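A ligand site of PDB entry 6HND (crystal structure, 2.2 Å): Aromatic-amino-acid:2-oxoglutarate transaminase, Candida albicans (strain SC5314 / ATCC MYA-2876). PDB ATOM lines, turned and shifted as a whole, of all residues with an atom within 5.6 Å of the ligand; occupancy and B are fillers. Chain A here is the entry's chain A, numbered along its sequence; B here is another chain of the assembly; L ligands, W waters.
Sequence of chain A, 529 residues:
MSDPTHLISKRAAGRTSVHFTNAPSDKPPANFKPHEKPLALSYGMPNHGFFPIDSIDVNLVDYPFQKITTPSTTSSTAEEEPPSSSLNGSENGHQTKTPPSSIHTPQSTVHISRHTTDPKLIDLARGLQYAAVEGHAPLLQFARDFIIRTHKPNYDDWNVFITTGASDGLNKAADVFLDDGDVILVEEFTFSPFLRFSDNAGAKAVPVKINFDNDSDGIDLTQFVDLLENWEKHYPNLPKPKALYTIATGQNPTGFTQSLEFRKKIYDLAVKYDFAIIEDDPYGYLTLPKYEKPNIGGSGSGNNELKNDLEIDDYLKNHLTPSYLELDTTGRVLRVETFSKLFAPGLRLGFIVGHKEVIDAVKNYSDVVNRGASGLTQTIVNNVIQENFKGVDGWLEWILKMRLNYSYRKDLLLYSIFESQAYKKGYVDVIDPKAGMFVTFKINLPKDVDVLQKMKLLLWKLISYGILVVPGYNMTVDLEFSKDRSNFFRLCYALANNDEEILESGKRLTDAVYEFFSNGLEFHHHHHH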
ATOM      1  N   THR A 164      17.277 -25.438   8.592  1.00  0.00           N
ATOM      2  CA  THR A 164      16.593 -25.212   9.885  1.00  0.00           C
ATOM      3  C   THR A 164      17.552 -25.471  11.047  1.00  0.00           C
ATOM      4  O   THR A 164      17.037 -25.709  12.134  1.00  0.00           O
ATOM      5  CB  THR A 164      15.287 -26.007   9.956  1.00  0.00           C
ATOM      6  OG1 THR A 164      15.497 -27.422   9.873  1.00  0.00           O
ATOM      7  CG2 THR A 164      14.366 -25.544   8.853  1.00  0.00           C
ATOM      8  N   GLY A 165      18.861 -25.385  10.824  1.00  0.00           N
ATOM      9  CA  GLY A 165      19.906 -25.571  11.857  1.00  0.00           C
ATOM     10  C   GLY A 165      21.006 -26.512  11.424  1.00  0.00           C
ATOM     11  O   GLY A 165      20.939 -27.007  10.302  1.00  0.00           O
ATOM     12  N   ALA A 166      21.994 -26.760  12.293  1.00  0.00           N
ATOM     13  CA  ALA A 166      23.146 -27.653  12.005  1.00  0.00           C
ATOM     14  C   ALA A 166      22.677 -29.104  11.836  1.00  0.00           C
ATOM     15  O   ALA A 166      23.095 -29.760  10.826  1.00  0.00           O
ATOM     16  CB  ALA A 166      24.185 -27.559  13.079  1.00  0.00           C
ATOM     17  N   SER A 167      21.808 -29.589  12.735  1.00  0.00           N
ATOM     18  CA  SER A 167      21.299 -30.986  12.628  1.00  0.00           C
ATOM     19  C   SER A 167      20.582 -31.166  11.287  1.00  0.00           C
ATOM     20  O   SER A 167      20.707 -32.255  10.711  1.00  0.00           O
ATOM     21  CB  SER A 167      20.413 -31.392  13.774  1.00  0.00           C
ATOM     22  OG  SER A 167      21.159 -31.491  14.979  1.00  0.00           O
ATOM     23  N   ASP A 168      19.885 -30.130  10.812  1.00  0.00           N
ATOM     24  CA  ASP A 168      19.212 -30.180   9.496  1.00  0.00           C
ATOM     25  C   ASP A 168      20.255 -30.232   8.357  1.00  0.00           C
ATOM     26  O   ASP A 168      20.101 -31.071   7.427  1.00  0.00           O
ATOM     27  CB  ASP A 168      18.233 -29.018   9.316  1.00  0.00           C
ATOM     28  CG  ASP A 168      17.425 -29.219   8.059  1.00  0.00           C
ATOM     29  OD1 ASP A 168      16.843 -30.305   7.915  1.00  0.00           O
ATOM     30  OD2 ASP A 168      17.445 -28.318   7.206  1.00  0.00           O
ATOM     31  N   LEU A 170      23.349 -31.279   8.603  1.00  0.00           N
ATOM     32  CA  LEU A 170      24.040 -32.570   8.742  1.00  0.00           C
ATOM     33  C   LEU A 170      23.216 -33.681   8.076  1.00  0.00           C
ATOM     34  O   LEU A 170      23.806 -34.578   7.426  1.00  0.00           O
ATOM     35  CB  LEU A 170      24.245 -32.848  10.237  1.00  0.00           C
ATOM     36  CG  LEU A 170      25.323 -32.054  10.962  1.00  0.00           C
ATOM     37  CD1 LEU A 170      25.422 -32.527  12.422  1.00  0.00           C
ATOM     38  CD2 LEU A 170      26.669 -32.201  10.266  1.00  0.00           C
ATOM     39  N   PHE A 191      28.978 -35.647  18.009  1.00  0.00           N
ATOM     40  CA  PHE A 191      27.578 -35.188  18.133  1.00  0.00           C
ATOM     41  C   PHE A 191      26.671 -36.361  17.702  1.00  0.00           C
ATOM     42  O   PHE A 191      26.399 -36.537  16.486  1.00  0.00           O
ATOM     43  CB  PHE A 191      27.417 -33.876  17.346  1.00  0.00           C
ATOM     44  CG  PHE A 191      26.006 -33.326  17.354  1.00  0.00           C
ATOM     45  CD1 PHE A 191      25.471 -32.803  18.513  1.00  0.00           C
ATOM     46  CD2 PHE A 191      25.216 -33.375  16.216  1.00  0.00           C
ATOM     47  CE1 PHE A 191      24.166 -32.314  18.535  1.00  0.00           C
ATOM     48  CE2 PHE A 191      23.931 -32.872  16.238  1.00  0.00           C
ATOM     49  CZ  PHE A 191      23.405 -32.334  17.395  1.00  0.00           C
ATOM     50  N   TYR A 245      33.004 -37.093   8.754  1.00  0.00           N
ATOM     51  CA  TYR A 245      32.255 -36.090   9.546  1.00  0.00           C
ATOM     52  C   TYR A 245      33.198 -35.620  10.653  1.00  0.00           C
ATOM     53  O   TYR A 245      33.594 -36.417  11.538  1.00  0.00           O
ATOM     54  CB  TYR A 245      30.938 -36.677  10.082  1.00  0.00           C
ATOM     55  CG  TYR A 245      30.272 -35.802  11.133  1.00  0.00           C
ATOM     56  CD1 TYR A 245      30.050 -34.463  10.875  1.00  0.00           C
ATOM     57  CD2 TYR A 245      29.858 -36.294  12.369  1.00  0.00           C
ATOM     58  CE1 TYR A 245      29.449 -33.634  11.806  1.00  0.00           C
ATOM     59  CE2 TYR A 245      29.246 -35.470  13.306  1.00  0.00           C
ATOM     60  CZ  TYR A 245      29.039 -34.131  13.028  1.00  0.00           C
ATOM     61  OH  TYR A 245      28.443 -33.269  13.885  1.00  0.00           O
ATOM     62  N   ILE A 247      33.973 -32.321  13.370  1.00  0.00           N
ATOM     63  CA  ILE A 247      33.729 -31.038  14.058  1.00  0.00           C
ATOM     64  C   ILE A 247      35.131 -30.512  14.374  1.00  0.00           C
ATOM     65  O   ILE A 247      35.570 -30.631  15.530  1.00  0.00           O
ATOM     66  CB  ILE A 247      32.853 -31.237  15.292  1.00  0.00           C
ATOM     67  CG1 ILE A 247      31.624 -32.089  14.992  1.00  0.00           C
ATOM     68  CG2 ILE A 247      32.458 -29.895  15.899  1.00  0.00           C
ATOM     69  CD1 ILE A 247      31.250 -33.037  16.122  1.00  0.00           C
ATOM     70  N   ASN A 252      32.922 -31.457  19.403  1.00  0.00           N
ATOM     71  CA  ASN A 252      31.918 -31.926  20.384  1.00  0.00           C
ATOM     72  C   ASN A 252      32.083 -33.447  20.523  1.00  0.00           C
ATOM     73  O   ASN A 252      31.784 -34.172  19.594  1.00  0.00           O
ATOM     74  CB  ASN A 252      30.539 -31.524  19.901  1.00  0.00           C
ATOM     75  CG  ASN A 252      29.476 -31.813  20.921  1.00  0.00           C
ATOM     76  OD1 ASN A 252      29.730 -32.531  21.893  1.00  0.00           O
ATOM     77  ND2 ASN A 252      28.298 -31.259  20.696  1.00  0.00           N
ATOM     78  N   ASP A 280      31.392 -29.591  10.267  1.00  0.00           N
ATOM     79  CA  ASP A 280      30.339 -29.026  11.162  1.00  0.00           C
ATOM     80  C   ASP A 280      31.020 -27.961  12.047  1.00  0.00           C
ATOM     81  O   ASP A 280      32.009 -28.333  12.712  1.00  0.00           O
ATOM     82  CB  ASP A 280      29.651 -30.155  11.919  1.00  0.00           C
ATOM     83  CG  ASP A 280      28.474 -29.764  12.797  1.00  0.00           C
ATOM     84  OD1 ASP A 280      27.983 -28.602  12.694  1.00  0.00           O
ATOM     85  OD2 ASP A 280      28.010 -30.662  13.562  1.00  0.00           O
ATOM     86  N   PRO A 282      29.481 -25.109  14.423  1.00  0.00           N
ATOM     87  CA  PRO A 282      28.518 -24.259  15.133  1.00  0.00           C
ATOM     88  C   PRO A 282      29.103 -23.143  16.011  1.00  0.00           C
ATOM     89  O   PRO A 282      28.377 -22.205  16.317  1.00  0.00           O
ATOM     90  CB  PRO A 282      27.755 -25.182  16.073  1.00  0.00           C
ATOM     91  CG  PRO A 282      28.241 -26.576  15.786  1.00  0.00           C
ATOM     92  CD  PRO A 282      29.526 -26.456  14.979  1.00  0.00           C
ATOM     93  N   TYR A 283      30.383 -23.236  16.395  1.00  0.00           N
ATOM     94  CA  TYR A 283      31.010 -22.227  17.310  1.00  0.00           C
ATOM     95  C   TYR A 283      32.516 -22.055  17.054  1.00  0.00           C
ATOM     96  O   TYR A 283      33.171 -21.501  17.907  1.00  0.00           O
ATOM     97  CB  TYR A 283      30.683 -22.587  18.770  1.00  0.00           C
ATOM     98  CG  TYR A 283      30.598 -24.071  18.988  1.00  0.00           C
ATOM     99  CD1 TYR A 283      31.589 -24.894  18.487  1.00  0.00           C
ATOM    100  CD2 TYR A 283      29.499 -24.657  19.603  1.00  0.00           C
ATOM    101  CE1 TYR A 283      31.477 -26.259  18.599  1.00  0.00           C
ATOM    102  CE2 TYR A 283      29.376 -26.028  19.721  1.00  0.00           C
ATOM    103  CZ  TYR A 283      30.368 -26.821  19.201  1.00  0.00           C
ATOM    104  OH  TYR A 283      30.345 -28.173  19.324  1.00  0.00           O
ATOM    105  N   THR A 338      25.111 -22.807  11.522  1.00  0.00           N
ATOM    106  CA  THR A 338      23.820 -22.610  12.230  1.00  0.00           C
ATOM    107  C   THR A 338      23.820 -21.229  12.856  1.00  0.00           C
ATOM    108  O   THR A 338      24.948 -20.678  13.140  1.00  0.00           O
ATOM    109  CB  THR A 338      23.553 -23.730  13.245  1.00  0.00           C
ATOM    110  OG1 THR A 338      22.357 -23.448  13.956  1.00  0.00           O
ATOM    111  CG2 THR A 338      24.651 -23.903  14.273  1.00  0.00           C
ATOM    112  N   PHE A 339      22.624 -20.724  13.099  1.00  0.00           N
ATOM    113  CA  PHE A 339      22.361 -19.487  13.885  1.00  0.00           C
ATOM    114  C   PHE A 339      22.080 -19.880  15.339  1.00  0.00           C
ATOM    115  O   PHE A 339      21.743 -18.960  16.130  1.00  0.00           O
ATOM    116  CB  PHE A 339      21.263 -18.640  13.219  1.00  0.00           C
ATOM    117  CG  PHE A 339      21.676 -18.022  11.896  1.00  0.00           C
ATOM    118  CD1 PHE A 339      22.542 -16.944  11.859  1.00  0.00           C
ATOM    119  CD2 PHE A 339      21.261 -18.552  10.688  1.00  0.00           C
ATOM    120  CE1 PHE A 339      22.941 -16.380  10.654  1.00  0.00           C
ATOM    121  CE2 PHE A 339      21.675 -18.014   9.474  1.00  0.00           C
ATOM    122  CZ  PHE A 339      22.515 -16.928   9.457  1.00  0.00           C
ATOM    123  N   SER A 340      22.207 -21.162  15.706  1.00  0.00           N
ATOM    124  CA  SER A 340      21.702 -21.708  16.999  1.00  0.00           C
ATOM    125  C   SER A 340      22.553 -21.167  18.155  1.00  0.00           C
ATOM    126  O   SER A 340      22.030 -20.819  19.212  1.00  0.00           O
ATOM    127  CB  SER A 340      21.655 -23.243  17.044  1.00  0.00           C
ATOM    128  OG  SER A 340      20.502 -23.787  16.398  1.00  0.00           O
ATOM    129  N   LYS A 341      23.882 -21.159  17.967  1.00  0.00           N
ATOM    130  CA  LYS A 341      24.807 -20.938  19.077  1.00  0.00           C
ATOM    131  C   LYS A 341      25.254 -19.462  19.074  1.00  0.00           C
ATOM    132  O   LYS A 341      25.627 -18.936  20.116  1.00  0.00           O
ATOM    133  CB  LYS A 341      25.879 -22.050  19.030  1.00  0.00           C
ATOM    134  CG  LYS A 341      25.331 -23.490  18.928  1.00  0.00           C
ATOM    135  CD  LYS A 341      25.384 -24.373  20.186  1.00  0.00           C
ATOM    136  CE  LYS A 341      24.644 -25.753  20.085  1.00  0.00           C
ATOM    137  NZ  LYS A 341      25.214 -26.617  19.041  1.00  0.00           N
ATOM    138  N   PRO A 345      19.125 -20.925  19.576  1.00  0.00           N
ATOM    139  CA  PRO A 345      18.673 -22.229  19.074  1.00  0.00           C
ATOM    140  C   PRO A 345      17.233 -22.226  18.537  1.00  0.00           C
ATOM    141  O   PRO A 345      16.898 -22.947  17.581  1.00  0.00           O
ATOM    142  CB  PRO A 345      18.794 -23.125  20.317  1.00  0.00           C
ATOM    143  CG  PRO A 345      19.804 -22.441  21.191  1.00  0.00           C
ATOM    144  CD  PRO A 345      19.565 -20.953  20.988  1.00  0.00           C
ATOM    145  N   ARG A 348      15.734 -22.235  14.772  1.00  0.00           N
ATOM    146  CA  ARG A 348      15.726 -23.372  13.832  1.00  0.00           C
ATOM    147  C   ARG A 348      16.136 -22.811  12.459  1.00  0.00           C
ATOM    148  O   ARG A 348      15.333 -22.862  11.499  1.00  0.00           O
ATOM    149  CB  ARG A 348      14.360 -24.079  13.774  1.00  0.00           C
ATOM    150  CG  ARG A 348      13.910 -24.714  15.092  1.00  0.00           C
ATOM    151  CD  ARG A 348      14.743 -25.890  15.573  1.00  0.00           C
ATOM    152  NE  ARG A 348      15.943 -25.470  16.248  1.00  0.00           N
ATOM    153  CZ  ARG A 348      17.079 -26.166  16.319  1.00  0.00           C
ATOM    154  NH1 ARG A 348      17.175 -27.364  15.776  1.00  0.00           N
ATOM    155  NH2 ARG A 348      18.130 -25.637  16.926  1.00  0.00           N
ATOM    156  N   LEU A 349      17.334 -22.236  12.410  1.00  0.00           N
ATOM    157  CA  LEU A 349      17.842 -21.574  11.184  1.00  0.00           C
ATOM    158  C   LEU A 349      19.339 -21.799  11.077  1.00  0.00           C
ATOM    159  O   LEU A 349      20.027 -21.674  12.094  1.00  0.00           O
ATOM    160  CB  LEU A 349      17.504 -20.089  11.251  1.00  0.00           C
ATOM    161  CG  LEU A 349      17.686 -19.343   9.931  1.00  0.00           C
ATOM    162  CD1 LEU A 349      16.733 -19.904   8.903  1.00  0.00           C
ATOM    163  CD2 LEU A 349      17.514 -17.842  10.119  1.00  0.00           C
ATOM    164  N   PHE A 438      32.719 -26.198  25.089  1.00  0.00           N
ATOM    165  CA  PHE A 438      32.865 -27.512  25.770  1.00  0.00           C
ATOM    166  C   PHE A 438      34.289 -27.687  26.313  1.00  0.00           C
ATOM    167  O   PHE A 438      35.248 -27.227  25.644  1.00  0.00           O
ATOM    168  CB  PHE A 438      32.504 -28.669  24.840  1.00  0.00           C
ATOM    169  CG  PHE A 438      31.071 -28.648  24.392  1.00  0.00           C
ATOM    170  CD1 PHE A 438      30.050 -28.600  25.320  1.00  0.00           C
ATOM    171  CD2 PHE A 438      30.752 -28.646  23.048  1.00  0.00           C
ATOM    172  CE1 PHE A 438      28.716 -28.545  24.919  1.00  0.00           C
ATOM    173  CE2 PHE A 438      29.433 -28.604  22.633  1.00  0.00           C
ATOM    174  CZ  PHE A 438      28.422 -28.555  23.563  1.00  0.00           C
ATOM    175  N   GLY B  44      24.340 -28.273  25.769  1.00  0.00           N
ATOM    176  CA  GLY B  44      24.952 -27.226  24.936  1.00  0.00           C
ATOM    177  C   GLY B  44      23.965 -26.125  24.557  1.00  0.00           C
ATOM    178  O   GLY B  44      23.828 -25.843  23.370  1.00  0.00           O
ATOM    179  N   TYR B 130      16.243 -24.078  22.802  1.00  0.00           N
ATOM    180  CA  TYR B 130      15.958 -25.495  22.461  1.00  0.00           C
ATOM    181  C   TYR B 130      14.641 -25.895  23.131  1.00  0.00           C
ATOM    182  O   TYR B 130      14.445 -25.566  24.335  1.00  0.00           O
ATOM    183  CB  TYR B 130      17.090 -26.424  22.894  1.00  0.00           C
ATOM    184  CG  TYR B 130      18.294 -26.434  21.964  1.00  0.00           C
ATOM    185  CD1 TYR B 130      18.206 -26.984  20.700  1.00  0.00           C
ATOM    186  CD2 TYR B 130      19.512 -25.897  22.350  1.00  0.00           C
ATOM    187  CE1 TYR B 130      19.287 -26.995  19.846  1.00  0.00           C
ATOM    188  CE2 TYR B 130      20.602 -25.899  21.502  1.00  0.00           C
ATOM    189  CZ  TYR B 130      20.504 -26.476  20.246  1.00  0.00           C
ATOM    190  OH  TYR B 130      21.576 -26.489  19.389  1.00  0.00           O
ATOM    191  N   ARG B 371      13.888 -31.394  12.669  1.00  0.00           N
ATOM    192  CA  ARG B 371      14.050 -31.312  14.155  1.00  0.00           C
ATOM    193  C   ARG B 371      13.392 -30.039  14.721  1.00  0.00           C
ATOM    194  O   ARG B 371      14.069 -29.250  15.397  1.00  0.00           O
ATOM    195  CB  ARG B 371      15.532 -31.437  14.531  1.00  0.00           C
ATOM    196  CG  ARG B 371      16.063 -32.841  14.315  1.00  0.00           C
ATOM    197  CD  ARG B 371      17.572 -32.894  14.303  1.00  0.00           C
ATOM    198  NE  ARG B 371      18.170 -32.618  15.621  1.00  0.00           N
ATOM    199  CZ  ARG B 371      18.243 -33.489  16.630  1.00  0.00           C
ATOM    200  NH1 ARG B 371      17.724 -34.695  16.487  1.00  0.00           N
ATOM    201  NH2 ARG B 371      18.797 -33.145  17.769  1.00  0.00           N
HETATM  202  N1  LIG L   1      26.746 -30.169  15.841  1.00  0.00           N
HETATM  203  C1  LIG L   1      27.413 -29.817  16.938  1.00  0.00           C
HETATM  204  C2  LIG L   1      28.855 -30.181  17.025  1.00  0.00           C
HETATM  205  C3  LIG L   1      26.778 -29.063  17.950  1.00  0.00           C
HETATM  206  O1  LIG L   1      27.518 -28.692  19.037  1.00  0.00           O
HETATM  207  C4  LIG L   1      25.410 -28.709  17.818  1.00  0.00           C
HETATM  208  C5  LIG L   1      24.792 -27.863  18.854  1.00  0.00           C
HETATM  209  C6  LIG L   1      24.740 -29.124  16.634  1.00  0.00           C
HETATM  210  C7  LIG L   1      25.442 -29.863  15.721  1.00  0.00           C
HETATM  211  C8  LIG L   1      23.274 -28.898  16.365  1.00  0.00           C
HETATM  212  O2  LIG L   1      22.882 -27.507  16.187  1.00  0.00           O
HETATM  213  P1  LIG L   1      21.395 -27.058  15.750  1.00  0.00           P
HETATM  214  O3  LIG L   1      21.604 -25.755  14.978  1.00  0.00           O
HETATM  215  O4  LIG L   1      20.624 -26.841  17.021  1.00  0.00           O
HETATM  216  O5  LIG L   1      20.798 -28.216  14.939  1.00  0.00           O
HETATM  217  O   HOH W   1      18.835 -28.398  12.908  1.00  0.00           O
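NZ of Lys 341 is covalently linked to C5 of the ligand (1.3 Å).
The side-chain hydroxyl (OH) of Tyr 130 of chain B sits at hydrogen-bond distance from an oxygen (O4) of the ligand, at 2.6 Å.
The side-chain hydroxyl of Thr 338 sits at hydrogen-bond distance from an oxygen (O3) of the ligand.
The side-chain carboxylate (OD2) of Asp 280 is in hydrogen-bond range of a nitrogen (N1) of the ligand (2.7 Å).
O3 of the ligand lies within hydrogen-bond range of OG of Ser 340 (2.7 Å).
The guanidinium group (NH2) of Arg 348 lies within salt-bridge range of an oxygen (O4) of the ligand, at 2.8 Å.
N of Ser 167 lies within hydrogen-bond range of O5 of the ligand.
An oxygen (O5) of the ligand is in hydrogen-bond range of the side-chain hydroxyl of Ser 167, at 3.3 Å.
OH of Tyr 283 lies within hydrogen-bond range of O1 of the ligand.
The backbone NH (N) of Ala 166 lies within hydrogen-bond range of an oxygen (O3) of the ligand, at 2.9 Å.
The side-chain amide nitrogen of Asn 252 is in hydrogen-bond range of an oxygen (O1) of the ligand.
The side-chain hydroxyl of Thr 338 lies within hydrogen-bond range of the backbone NH of Ser 340.
OG1 of Thr 338 is in hydrogen-bond range of O of Leu 349 (3.5 Å).
The side-chain carboxylate (OD2) of Asp 280 sits at hydrogen-bond distance from the side-chain hydroxyl (OH) of Tyr 245 (2.7 Å).
NH2 of Arg 348 lies within hydrogen-bond range of OG of Ser 340 (3.1 Å).
The backbone carbonyl oxygen (O) of Pro 345 is in hydrogen-bond range of the guanidinium group (NE) of Arg 348, 3.0 Å away.
OG of Ser 167 sits close to NE of Arg 371 of chain B, 3.3 Å away.
CA of Gly 165 touches O3 of the ligand, 3.6 Å away.
Phe 191 touches the ligand.
CG2 of Ile 247 touches C2 of the ligand, 3.8 Å away.
CG of Pro 282 touches C1 of the ligand, 3.5 Å away.
Hydrophobic or aromatic side chains within 4 Å of the ligand: Ala 166, Phe 191, Ile 247, Pro 282, Tyr 283 and Tyr 130 of chain B.
The nearest printed residue that does not touch the ligand is Tyr 245 (4.04 Å).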
